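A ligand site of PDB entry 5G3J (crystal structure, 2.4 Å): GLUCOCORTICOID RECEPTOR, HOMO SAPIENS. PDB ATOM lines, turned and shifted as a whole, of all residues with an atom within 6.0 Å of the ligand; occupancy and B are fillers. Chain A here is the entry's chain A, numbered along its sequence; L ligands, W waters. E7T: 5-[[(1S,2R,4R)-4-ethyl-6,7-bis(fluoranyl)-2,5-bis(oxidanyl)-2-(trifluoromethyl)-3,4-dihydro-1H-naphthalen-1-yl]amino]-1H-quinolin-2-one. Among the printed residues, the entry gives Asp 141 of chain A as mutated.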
ATOM      1  N   ILE A  62      20.554  18.566 -13.168  1.00  0.00           N
ATOM      2  CA  ILE A  62      19.374  19.398 -13.452  1.00  0.00           C
ATOM      3  C   ILE A  62      18.561  19.639 -12.174  1.00  0.00           C
ATOM      4  O   ILE A  62      18.201  20.794 -11.901  1.00  0.00           O
ATOM      5  CB  ILE A  62      18.535  18.810 -14.626  1.00  0.00           C
ATOM      6  CG1 ILE A  62      19.328  18.947 -15.962  1.00  0.00           C
ATOM      7  CG2 ILE A  62      17.129  19.459 -14.703  1.00  0.00           C
ATOM      8  CD1 ILE A  62      18.731  18.301 -17.142  1.00  0.00           C
ATOM      9  N   MET A  63      18.327  18.586 -11.378  1.00  0.00           N
ATOM     10  CA  MET A  63      17.597  18.676 -10.109  1.00  0.00           C
ATOM     11  C   MET A  63      18.259  19.657  -9.154  1.00  0.00           C
ATOM     12  O   MET A  63      17.590  20.541  -8.618  1.00  0.00           O
ATOM     13  CB  MET A  63      17.416  17.287  -9.460  1.00  0.00           C
ATOM     14  CG  MET A  63      16.360  16.440 -10.161  1.00  0.00           C
ATOM     15  SD  MET A  63      16.147  14.765  -9.461  1.00  0.00           S
ATOM     16  CE  MET A  63      15.482  15.172  -7.862  1.00  0.00           C
ATOM     17  N   LEU A  66      18.002  23.259 -10.434  1.00  0.00           N
ATOM     18  CA  LEU A  66      16.615  23.691 -10.237  1.00  0.00           C
ATOM     19  C   LEU A  66      16.319  24.060  -8.783  1.00  0.00           C
ATOM     20  O   LEU A  66      15.644  25.056  -8.548  1.00  0.00           O
ATOM     21  CB  LEU A  66      15.595  22.679 -10.790  1.00  0.00           C
ATOM     22  CG  LEU A  66      15.557  22.511 -12.328  1.00  0.00           C
ATOM     23  CD1 LEU A  66      14.510  21.518 -12.744  1.00  0.00           C
ATOM     24  CD2 LEU A  66      15.345  23.824 -13.041  1.00  0.00           C
ATOM     25  N   ASN A  67      16.914  23.316  -7.818  1.00  0.00           N
ATOM     26  CA  ASN A  67      16.784  23.619  -6.395  1.00  0.00           C
ATOM     27  C   ASN A  67      17.372  24.992  -6.083  1.00  0.00           C
ATOM     28  O   ASN A  67      16.705  25.776  -5.407  1.00  0.00           O
ATOM     29  CB  ASN A  67      17.446  22.543  -5.520  1.00  0.00           C
ATOM     30  CG  ASN A  67      16.708  21.228  -5.508  1.00  0.00           C
ATOM     31  OD1 ASN A  67      15.572  21.122  -5.954  1.00  0.00           O
ATOM     32  ND2 ASN A  67      17.325  20.214  -4.942  1.00  0.00           N
ATOM     33  N   MET A  68      18.576  25.304  -6.614  1.00  0.00           N
ATOM     34  CA  MET A  68      19.265  26.594  -6.417  1.00  0.00           C
ATOM     35  C   MET A  68      18.485  27.751  -7.054  1.00  0.00           C
ATOM     36  O   MET A  68      18.324  28.787  -6.433  1.00  0.00           O
ATOM     37  CB  MET A  68      20.736  26.566  -6.883  1.00  0.00           C
ATOM     38  CG  MET A  68      21.593  25.482  -6.206  1.00  0.00           C
ATOM     39  SD  MET A  68      21.688  25.576  -4.385  1.00  0.00           S
ATOM     40  CE  MET A  68      21.634  23.836  -3.996  1.00  0.00           C
ATOM     41  N   LEU A  69      17.920  27.521  -8.246  1.00  0.00           N
ATOM     42  CA  LEU A  69      17.074  28.491  -8.939  1.00  0.00           C
ATOM     43  C   LEU A  69      15.792  28.757  -8.135  1.00  0.00           C
ATOM     44  O   LEU A  69      15.413  29.921  -7.975  1.00  0.00           O
ATOM     45  CB  LEU A  69      16.735  27.996 -10.365  1.00  0.00           C
ATOM     46  CG  LEU A  69      15.923  28.958 -11.259  1.00  0.00           C
ATOM     47  CD1 LEU A  69      16.637  30.322 -11.434  1.00  0.00           C
ATOM     48  CD2 LEU A  69      15.643  28.310 -12.616  1.00  0.00           C
ATOM     49  N   GLY A  70      15.171  27.684  -7.630  1.00  0.00           N
ATOM     50  CA  GLY A  70      13.947  27.741  -6.847  1.00  0.00           C
ATOM     51  C   GLY A  70      14.095  28.601  -5.611  1.00  0.00           C
ATOM     52  O   GLY A  70      13.176  29.380  -5.288  1.00  0.00           O
ATOM     53  N   GLY A  71      15.235  28.470  -4.926  1.00  0.00           N
ATOM     54  CA  GLY A  71      15.569  29.263  -3.746  1.00  0.00           C
ATOM     55  C   GLY A  71      15.651  30.737  -4.087  1.00  0.00           C
ATOM     56  O   GLY A  71      15.112  31.568  -3.341  1.00  0.00           O
ATOM     57  N   GLN A  73      14.155  32.097  -6.717  1.00  0.00           N
ATOM     58  CA  GLN A  73      12.797  32.474  -7.110  1.00  0.00           C
ATOM     59  C   GLN A  73      11.937  32.759  -5.885  1.00  0.00           C
ATOM     60  O   GLN A  73      11.108  33.679  -5.919  1.00  0.00           O
ATOM     61  CB  GLN A  73      12.140  31.405  -7.978  1.00  0.00           C
ATOM     62  CG  GLN A  73      12.702  31.361  -9.396  1.00  0.00           C
ATOM     63  CD  GLN A  73      12.130  32.389 -10.351  1.00  0.00           C
ATOM     64  OE1 GLN A  73      11.547  33.429  -9.962  1.00  0.00           O
ATOM     65  NE2 GLN A  73      12.309  32.132 -11.624  1.00  0.00           N
ATOM     66  N   TRP A 103       4.255  28.263  -1.822  1.00  0.00           N
ATOM     67  CA  TRP A 103       5.541  28.362  -2.547  1.00  0.00           C
ATOM     68  C   TRP A 103       5.592  27.546  -3.868  1.00  0.00           C
ATOM     69  O   TRP A 103       5.871  28.130  -4.918  1.00  0.00           O
ATOM     70  CB  TRP A 103       6.720  28.021  -1.624  1.00  0.00           C
ATOM     71  CG  TRP A 103       6.886  26.575  -1.275  1.00  0.00           C
ATOM     72  CD1 TRP A 103       6.091  25.819  -0.470  1.00  0.00           C
ATOM     73  CD2 TRP A 103       7.909  25.692  -1.774  1.00  0.00           C
ATOM     74  NE1 TRP A 103       6.557  24.522  -0.426  1.00  0.00           N
ATOM     75  CE2 TRP A 103       7.688  24.429  -1.195  1.00  0.00           C
ATOM     76  CE3 TRP A 103       9.005  25.866  -2.636  1.00  0.00           C
ATOM     77  CZ2 TRP A 103       8.528  23.339  -1.437  1.00  0.00           C
ATOM     78  CZ3 TRP A 103       9.818  24.777  -2.898  1.00  0.00           C
ATOM     79  CH2 TRP A 103       9.587  23.535  -2.304  1.00  0.00           C
ATOM     80  N   MET A 104       5.264  26.222  -3.819  1.00  0.00           N
ATOM     81  CA  MET A 104       5.314  25.321  -4.972  1.00  0.00           C
ATOM     82  C   MET A 104       4.225  25.693  -5.994  1.00  0.00           C
ATOM     83  O   MET A 104       4.479  25.657  -7.200  1.00  0.00           O
ATOM     84  CB  MET A 104       5.194  23.849  -4.516  1.00  0.00           C
ATOM     85  CG  MET A 104       5.420  22.820  -5.648  1.00  0.00           C
ATOM     86  SD  MET A 104       7.071  22.944  -6.387  1.00  0.00           S
ATOM     87  CE  MET A 104       7.979  21.888  -5.248  1.00  0.00           C
ATOM     88  N   MET A 107       5.416  28.883  -7.846  1.00  0.00           N
ATOM     89  CA  MET A 107       6.517  28.546  -8.737  1.00  0.00           C
ATOM     90  C   MET A 107       6.086  27.769  -9.963  1.00  0.00           C
ATOM     91  O   MET A 107       6.533  28.087 -11.065  1.00  0.00           O
ATOM     92  CB  MET A 107       7.617  27.821  -7.982  1.00  0.00           C
ATOM     93  CG  MET A 107       8.308  28.722  -6.988  1.00  0.00           C
ATOM     94  SD  MET A 107      10.023  28.286  -6.795  1.00  0.00           S
ATOM     95  CE  MET A 107       9.891  26.516  -6.376  1.00  0.00           C
ATOM     96  N   ALA A 108       5.242  26.743  -9.774  1.00  0.00           N
ATOM     97  CA  ALA A 108       4.749  25.896 -10.854  1.00  0.00           C
ATOM     98  C   ALA A 108       3.847  26.701 -11.783  1.00  0.00           C
ATOM     99  O   ALA A 108       3.946  26.562 -13.000  1.00  0.00           O
ATOM    100  CB  ALA A 108       4.014  24.677 -10.288  1.00  0.00           C
ATOM    101  N   LEU A 111       6.012  29.141 -13.846  1.00  0.00           N
ATOM    102  CA  LEU A 111       6.703  28.299 -14.825  1.00  0.00           C
ATOM    103  C   LEU A 111       5.777  27.905 -15.976  1.00  0.00           C
ATOM    104  O   LEU A 111       6.171  27.987 -17.135  1.00  0.00           O
ATOM    105  CB  LEU A 111       7.287  27.041 -14.139  1.00  0.00           C
ATOM    106  CG  LEU A 111       7.732  25.895 -15.054  1.00  0.00           C
ATOM    107  CD1 LEU A 111       9.010  26.253 -15.820  1.00  0.00           C
ATOM    108  CD2 LEU A 111       7.897  24.645 -14.279  1.00  0.00           C
ATOM    109  N   ARG A 114       5.442  31.028 -18.157  1.00  0.00           N
ATOM    110  CA  ARG A 114       6.657  31.272 -18.975  1.00  0.00           C
ATOM    111  C   ARG A 114       6.686  30.294 -20.137  1.00  0.00           C
ATOM    112  O   ARG A 114       7.000  30.688 -21.251  1.00  0.00           O
ATOM    113  CB  ARG A 114       7.957  31.014 -18.190  1.00  0.00           C
ATOM    114  CG  ARG A 114       8.240  31.953 -17.064  1.00  0.00           C
ATOM    115  CD  ARG A 114       9.727  31.948 -16.688  1.00  0.00           C
ATOM    116  NE  ARG A 114      10.195  30.801 -15.893  1.00  0.00           N
ATOM    117  CZ  ARG A 114       9.949  30.595 -14.595  1.00  0.00           C
ATOM    118  NH1 ARG A 114       9.110  31.387 -13.927  1.00  0.00           N
ATOM    119  NH2 ARG A 114      10.495  29.568 -13.967  1.00  0.00           N
ATOM    120  N   LEU A 124       9.484  22.960 -20.847  1.00  0.00           N
ATOM    121  CA  LEU A 124       9.433  23.638 -19.554  1.00  0.00           C
ATOM    122  C   LEU A 124      10.524  24.699 -19.566  1.00  0.00           C
ATOM    123  O   LEU A 124      11.716  24.371 -19.671  1.00  0.00           O
ATOM    124  CB  LEU A 124       9.581  22.672 -18.369  1.00  0.00           C
ATOM    125  CG  LEU A 124       8.342  21.844 -17.975  1.00  0.00           C
ATOM    126  CD1 LEU A 124       8.663  20.949 -16.812  1.00  0.00           C
ATOM    127  CD2 LEU A 124       7.141  22.743 -17.604  1.00  0.00           C
ATOM    128  N   PHE A 126      12.225  26.932 -17.460  1.00  0.00           N
ATOM    129  CA  PHE A 126      12.626  27.313 -16.107  1.00  0.00           C
ATOM    130  C   PHE A 126      13.340  28.658 -16.098  1.00  0.00           C
ATOM    131  O   PHE A 126      12.987  29.548 -15.337  1.00  0.00           O
ATOM    132  CB  PHE A 126      13.486  26.215 -15.459  1.00  0.00           C
ATOM    133  CG  PHE A 126      12.682  25.026 -15.004  1.00  0.00           C
ATOM    134  CD1 PHE A 126      12.038  25.033 -13.771  1.00  0.00           C
ATOM    135  CD2 PHE A 126      12.588  23.882 -15.787  1.00  0.00           C
ATOM    136  CE1 PHE A 126      11.308  23.917 -13.330  1.00  0.00           C
ATOM    137  CE2 PHE A 126      11.848  22.782 -15.363  1.00  0.00           C
ATOM    138  CZ  PHE A 126      11.203  22.808 -14.142  1.00  0.00           C
ATOM    139  N   ILE A 132      13.858  22.620 -20.510  1.00  0.00           N
ATOM    140  CA  ILE A 132      13.834  21.180 -20.514  1.00  0.00           C
ATOM    141  C   ILE A 132      13.112  20.731 -21.790  1.00  0.00           C
ATOM    142  O   ILE A 132      11.885  20.797 -21.913  1.00  0.00           O
ATOM    143  CB  ILE A 132      13.355  20.569 -19.158  1.00  0.00           C
ATOM    144  CG1 ILE A 132      14.442  20.887 -18.082  1.00  0.00           C
ATOM    145  CG2 ILE A 132      13.098  19.044 -19.276  1.00  0.00           C
ATOM    146  CD1 ILE A 132      14.101  20.648 -16.696  1.00  0.00           C
ATOM    147  N   ASP A 141      13.946   9.345 -15.081  1.00  0.00           N
ATOM    148  CA  ASP A 141      12.866   9.893 -14.247  1.00  0.00           C
ATOM    149  C   ASP A 141      12.657  11.427 -14.397  1.00  0.00           C
ATOM    150  O   ASP A 141      12.034  12.047 -13.530  1.00  0.00           O
ATOM    151  CB  ASP A 141      13.025   9.498 -12.757  1.00  0.00           C
ATOM    152  CG  ASP A 141      11.713   9.369 -11.996  1.00  0.00           C
ATOM    153  OD1 ASP A 141      10.961   8.377 -12.257  1.00  0.00           O
ATOM    154  OD2 ASP A 141      11.439  10.222 -11.117  1.00  0.00           O
ATOM    155  N   MET A 142      13.090  12.008 -15.522  1.00  0.00           N
ATOM    156  CA  MET A 142      12.871  13.433 -15.759  1.00  0.00           C
ATOM    157  C   MET A 142      11.404  13.714 -16.105  1.00  0.00           C
ATOM    158  O   MET A 142      10.824  14.659 -15.555  1.00  0.00           O
ATOM    159  CB  MET A 142      13.824  13.995 -16.840  1.00  0.00           C
ATOM    160  CG  MET A 142      13.930  15.525 -16.828  1.00  0.00           C
ATOM    161  SD  MET A 142      14.460  16.236 -15.252  1.00  0.00           S
ATOM    162  CE  MET A 142      16.139  15.775 -15.229  1.00  0.00           C
ATOM    163  N   GLN A 145       8.558  13.700 -13.164  1.00  0.00           N
ATOM    164  CA  GLN A 145       8.498  14.903 -12.345  1.00  0.00           C
ATOM    165  C   GLN A 145       8.075  16.150 -13.156  1.00  0.00           C
ATOM    166  O   GLN A 145       7.450  17.046 -12.595  1.00  0.00           O
ATOM    167  CB  GLN A 145       9.794  15.163 -11.542  1.00  0.00           C
ATOM    168  CG  GLN A 145      11.112  14.783 -12.204  1.00  0.00           C
ATOM    169  CD  GLN A 145      12.189  14.480 -11.193  1.00  0.00           C
ATOM    170  OE1 GLN A 145      12.220  15.045 -10.105  1.00  0.00           O
ATOM    171  NE2 GLN A 145      13.108  13.600 -11.505  1.00  0.00           N
ATOM    172  N   CYS A 146       8.341  16.160 -14.468  1.00  0.00           N
ATOM    173  CA  CYS A 146       8.017  17.264 -15.378  1.00  0.00           C
ATOM    174  C   CYS A 146       6.567  17.284 -15.882  1.00  0.00           C
ATOM    175  O   CYS A 146       6.042  18.367 -16.147  1.00  0.00           O
ATOM    176  CB  CYS A 146       9.002  17.280 -16.549  1.00  0.00           C
ATOM    177  SG  CYS A 146      10.645  17.893 -16.121  1.00  0.00           S
ATOM    178  N   MET A 149       3.965  19.651 -14.311  1.00  0.00           N
ATOM    179  CA  MET A 149       4.247  21.042 -14.638  1.00  0.00           C
ATOM    180  C   MET A 149       3.859  21.308 -16.088  1.00  0.00           C
ATOM    181  O   MET A 149       3.272  22.356 -16.370  1.00  0.00           O
ATOM    182  CB  MET A 149       5.716  21.383 -14.336  1.00  0.00           C
ATOM    183  CG  MET A 149       6.004  21.435 -12.849  1.00  0.00           C
ATOM    184  SD  MET A 149       7.760  21.662 -12.446  1.00  0.00           S
ATOM    185  CE  MET A 149       8.404  20.093 -12.855  1.00  0.00           C
ATOM    186  N   LEU A 235       4.618  17.246  -6.864  1.00  0.00           N
ATOM    187  CA  LEU A 235       5.922  17.917  -6.803  1.00  0.00           C
ATOM    188  C   LEU A 235       6.512  17.881  -5.383  1.00  0.00           C
ATOM    189  O   LEU A 235       7.714  17.711  -5.236  1.00  0.00           O
ATOM    190  CB  LEU A 235       5.820  19.367  -7.323  1.00  0.00           C
ATOM    191  CG  LEU A 235       5.347  19.553  -8.782  1.00  0.00           C
ATOM    192  CD1 LEU A 235       4.920  20.985  -9.050  1.00  0.00           C
ATOM    193  CD2 LEU A 235       6.437  19.125  -9.774  1.00  0.00           C
ATOM    194  N   TYR A 238       8.285  14.380  -4.408  1.00  0.00           N
ATOM    195  CA  TYR A 238       9.678  14.326  -4.878  1.00  0.00           C
ATOM    196  C   TYR A 238      10.542  15.203  -3.970  1.00  0.00           C
ATOM    197  O   TYR A 238      11.592  14.791  -3.500  1.00  0.00           O
ATOM    198  CB  TYR A 238       9.804  14.832  -6.334  1.00  0.00           C
ATOM    199  CG  TYR A 238       9.380  13.830  -7.374  1.00  0.00           C
ATOM    200  CD1 TYR A 238      10.218  12.789  -7.750  1.00  0.00           C
ATOM    201  CD2 TYR A 238       8.155  13.960  -8.025  1.00  0.00           C
ATOM    202  CE1 TYR A 238       9.828  11.866  -8.723  1.00  0.00           C
ATOM    203  CE2 TYR A 238       7.755  13.035  -9.001  1.00  0.00           C
ATOM    204  CZ  TYR A 238       8.595  11.990  -9.343  1.00  0.00           C
ATOM    205  OH  TYR A 238       8.215  11.065 -10.280  1.00  0.00           O
ATOM    206  N   CYS A 239      10.035  16.392  -3.698  1.00  0.00           N
ATOM    207  CA  CYS A 239      10.650  17.407  -2.859  1.00  0.00           C
ATOM    208  C   CYS A 239      11.023  16.922  -1.466  1.00  0.00           C
ATOM    209  O   CYS A 239      12.198  17.003  -1.089  1.00  0.00           O
ATOM    210  CB  CYS A 239       9.722  18.604  -2.797  1.00  0.00           C
ATOM    211  SG  CYS A 239      10.575  20.160  -2.912  1.00  0.00           S
ATOM    212  N   THR A 242      13.659  13.757  -1.590  1.00  0.00           N
ATOM    213  CA  THR A 242      15.022  14.202  -1.942  1.00  0.00           C
ATOM    214  C   THR A 242      15.656  15.018  -0.841  1.00  0.00           C
ATOM    215  O   THR A 242      16.860  14.895  -0.603  1.00  0.00           O
ATOM    216  CB  THR A 242      15.048  14.926  -3.286  1.00  0.00           C
ATOM    217  OG1 THR A 242      14.214  16.072  -3.207  1.00  0.00           O
ATOM    218  CG2 THR A 242      14.588  14.051  -4.447  1.00  0.00           C
ATOM    219  N   ILE A 250      21.274  15.404  -2.693  1.00  0.00           N
ATOM    220  CA  ILE A 250      20.503  16.442  -3.368  1.00  0.00           C
ATOM    221  C   ILE A 250      20.362  17.622  -2.414  1.00  0.00           C
ATOM    222  O   ILE A 250      19.670  17.541  -1.401  1.00  0.00           O
ATOM    223  CB  ILE A 250      19.171  15.927  -3.997  1.00  0.00           C
ATOM    224  CG1 ILE A 250      19.487  15.171  -5.318  1.00  0.00           C
ATOM    225  CG2 ILE A 250      18.205  17.091  -4.263  1.00  0.00           C
ATOM    226  CD1 ILE A 250      18.452  14.180  -5.740  1.00  0.00           C
ATOM    227  N   PHE A 252      19.493  21.472  -1.157  1.00  0.00           N
ATOM    228  CA  PHE A 252      18.484  22.503  -1.254  1.00  0.00           C
ATOM    229  C   PHE A 252      19.097  23.768  -0.634  1.00  0.00           C
ATOM    230  O   PHE A 252      19.772  23.671   0.397  1.00  0.00           O
ATOM    231  CB  PHE A 252      17.193  22.105  -0.520  1.00  0.00           C
ATOM    232  CG  PHE A 252      16.354  21.122  -1.291  1.00  0.00           C
ATOM    233  CD1 PHE A 252      16.645  19.758  -1.258  1.00  0.00           C
ATOM    234  CD2 PHE A 252      15.248  21.539  -2.026  1.00  0.00           C
ATOM    235  CE1 PHE A 252      15.858  18.846  -1.976  1.00  0.00           C
ATOM    236  CE2 PHE A 252      14.451  20.630  -2.716  1.00  0.00           C
ATOM    237  CZ  PHE A 252      14.775  19.280  -2.695  1.00  0.00           C
ATOM    238  N   LEU A 256      14.662  27.172   0.586  1.00  0.00           N
ATOM    239  CA  LEU A 256      13.854  25.996   0.336  1.00  0.00           C
ATOM    240  C   LEU A 256      13.924  25.017   1.474  1.00  0.00           C
ATOM    241  O   LEU A 256      12.871  24.507   1.887  1.00  0.00           O
ATOM    242  CB  LEU A 256      14.218  25.329  -0.999  1.00  0.00           C
ATOM    243  CG  LEU A 256      13.996  26.188  -2.241  1.00  0.00           C
ATOM    244  CD1 LEU A 256      14.000  25.335  -3.489  1.00  0.00           C
ATOM    245  CD2 LEU A 256      12.701  27.015  -2.128  1.00  0.00           C
ATOM    246  N   ILE A 260      10.642  23.604   3.478  1.00  0.00           N
ATOM    247  CA  ILE A 260      10.390  22.150   3.524  1.00  0.00           C
ATOM    248  C   ILE A 260      10.371  21.652   4.974  1.00  0.00           C
ATOM    249  O   ILE A 260       9.451  20.913   5.351  1.00  0.00           O
ATOM    250  CB  ILE A 260      11.377  21.371   2.586  1.00  0.00           C
ATOM    251  CG1 ILE A 260      11.223  21.843   1.122  1.00  0.00           C
ATOM    252  CG2 ILE A 260      11.154  19.868   2.680  1.00  0.00           C
ATOM    253  CD1 ILE A 260      12.384  21.496   0.220  1.00  0.00           C
HETATM  254  C1  E7T L   1      13.164  17.329  -5.905  1.00  0.00           C
HETATM  255  C2  E7T L   1      12.091  18.059  -6.716  1.00  0.00           C
HETATM  256  C3  E7T L   1      12.752  19.268  -7.381  1.00  0.00           C
HETATM  257  C5  E7T L   1      12.434  20.492  -6.515  1.00  0.00           C
HETATM  258  C6  E7T L   1      12.536  21.825  -7.281  1.00  0.00           C
HETATM  259  O7  E7T L   1      13.846  21.999  -7.835  1.00  0.00           O
HETATM  260  C8  E7T L   1      11.478  21.812  -8.411  1.00  0.00           C
HETATM  261  N10 E7T L   1      11.716  23.035  -9.182  1.00  0.00           N
HETATM  262  C11 E7T L   1      10.716  23.911  -9.589  1.00  0.00           C
HETATM  263  C12 E7T L   1       9.367  23.516  -9.620  1.00  0.00           C
HETATM  264  C13 E7T L   1       8.403  24.400 -10.080  1.00  0.00           C
HETATM  265  C14 E7T L   1       8.760  25.667 -10.548  1.00  0.00           C
HETATM  266  C15 E7T L   1      10.087  26.077 -10.526  1.00  0.00           C
HETATM  267  N16 E7T L   1      10.452  27.338 -10.980  1.00  0.00           N
HETATM  268  C18 E7T L   1      11.736  27.755 -10.932  1.00  0.00           C
HETATM  269  O19 E7T L   1      12.012  28.873 -11.337  1.00  0.00           O
HETATM  270  C20 E7T L   1      12.756  26.904 -10.403  1.00  0.00           C
HETATM  271  C21 E7T L   1      12.450  25.651  -9.972  1.00  0.00           C
HETATM  272  C22 E7T L   1      11.097  25.210 -10.021  1.00  0.00           C
HETATM  273  C23 E7T L   1      11.736  20.612  -9.311  1.00  0.00           C
HETATM  274  C24 E7T L   1      11.453  20.736 -10.677  1.00  0.00           C
HETATM  275  C25 E7T L   1      11.769  19.725 -11.566  1.00  0.00           C
HETATM  276  F26 E7T L   1      11.493  19.848 -12.887  1.00  0.00           F
HETATM  277  C27 E7T L   1      12.404  18.588 -11.130  1.00  0.00           C
HETATM  278  F28 E7T L   1      12.706  17.618 -12.007  1.00  0.00           F
HETATM  279  C29 E7T L   1      12.716  18.447  -9.774  1.00  0.00           C
HETATM  280  O30 E7T L   1      13.333  17.310  -9.386  1.00  0.00           O
HETATM  281  C31 E7T L   1      12.357  19.447  -8.845  1.00  0.00           C
HETATM  282  C32 E7T L   1      12.322  22.987  -6.287  1.00  0.00           C
HETATM  283  F33 E7T L   1      13.183  22.810  -5.205  1.00  0.00           F
HETATM  284  F34 E7T L   1      12.639  24.217  -6.872  1.00  0.00           F
HETATM  285  F35 E7T L   1      11.004  23.022  -5.832  1.00  0.00           F
HETATM  286  O   HOH W   1       8.746  29.699 -11.396  1.00  0.00           O
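NH2 of Arg 114 lies within hydrogen-bond range of O of Phe 126 (2.8 Å).
The side-chain sulfur (SG) of Cys 146 lies within hydrogen-bond range of the backbone carbonyl oxygen (O) of Met 142.
The side-chain hydroxyl (OH) of Tyr 238 sits close to the side-chain carboxylate (OD2) of Asp 141 (3.4 Å).
The side-chain hydroxyl (OG1) of Thr 242 sits at hydrogen-bond distance from the backbone carbonyl oxygen (O) of Cys 239 (3.1 Å).
OG1 of Thr 242 lies within hydrogen-bond range of O of Tyr 238 (2.9 Å).
The side-chain amide nitrogen of Gln 145 is in hydrogen-bond range of the backbone carbonyl oxygen of Asp 141.
The backbone carbonyl oxygen of Met 63 sits close to the side-chain amide oxygen of Asn 67 (3.4 Å).
SD of Met 63 sits close to O30 of the ligand, 3.8 Å away.
NH2 of Arg 114 lies within hydrogen-bond range of O19 of the ligand (3.1 Å).
An oxygen (O7) of the ligand is in hydrogen-bond range of the backbone NH (N) of Asn 67 (3.3 Å).
The side-chain amide oxygen of Asn 67 is in hydrogen-bond range of an oxygen (O7) of the ligand (2.7 Å).
The side-chain amide nitrogen (NE2) of Gln 73 lies close to an oxygen (O19) of the ligand (3.3 Å).
O30 of the ligand sits at hydrogen-bond distance from OE1 of Gln 145 (2.6 Å).
Leu 66 touches the ligand (C to O7, 3.4 Å).
Leu 69 touches the ligand.
Gly 70 touches the ligand.
CZ3 of Trp 103 touches F35 of the ligand, at 3.6 Å.
CE of Met 104 touches F35 of the ligand, 3.3 Å away.
O of Met 107 touches C14 of the ligand, at 3.3 Å.
N of Ala 108 touches C14 of the ligand (3.8 Å).
CD2 of Leu 111 touches C14 of the ligand, 3.96 Å away.
Phe 126 touches the ligand (CZ to F26, 3.2 Å).
Met 142 touches the ligand (SD to F28, 3.9 Å).
SG of Cys 146 touches F26 of the ligand (3.9 Å).
CE of Met 149 touches F26 of the ligand, 3.1 Å away.
Tyr 238 touches the ligand.
Cys 239 touches the ligand (N to C1, 3.9 Å).
Thr 242 touches the ligand.
CE2 of Phe 252 touches F33 of the ligand (3.5 Å).
Leu 256 touches the ligand (CD1 to F33, 3.2 Å).
Hydrophobic or aromatic side chains that line the ligand: Met 63, Leu 66, Leu 69, Trp 103, Met 104, Met 107, Leu 111, Phe 126, Met 142, Met 149, Tyr 238, Phe 252 and Leu 256.
Within 4 Å of the ligand: Met 63, Leu 66, Asn 67, Leu 69, Gly 70, Gln 73, Trp 103, Met 104, Met 107, Ala 108, Leu 111, Arg 114, Phe 126, Met 142, Gln 145, Cys 146, Met 149, Tyr 238, Cys 239, Thr 242, Phe 252 and Leu 256.
The nearest printed residue that does not touch the ligand is Leu 235 (4.6 Å).
Water W1 lies within hydrogen-bond range of O of Met 107 (2.8 Å), N16 of the ligand (2.9 Å) and NH1 of Arg 114 (3.1 Å).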
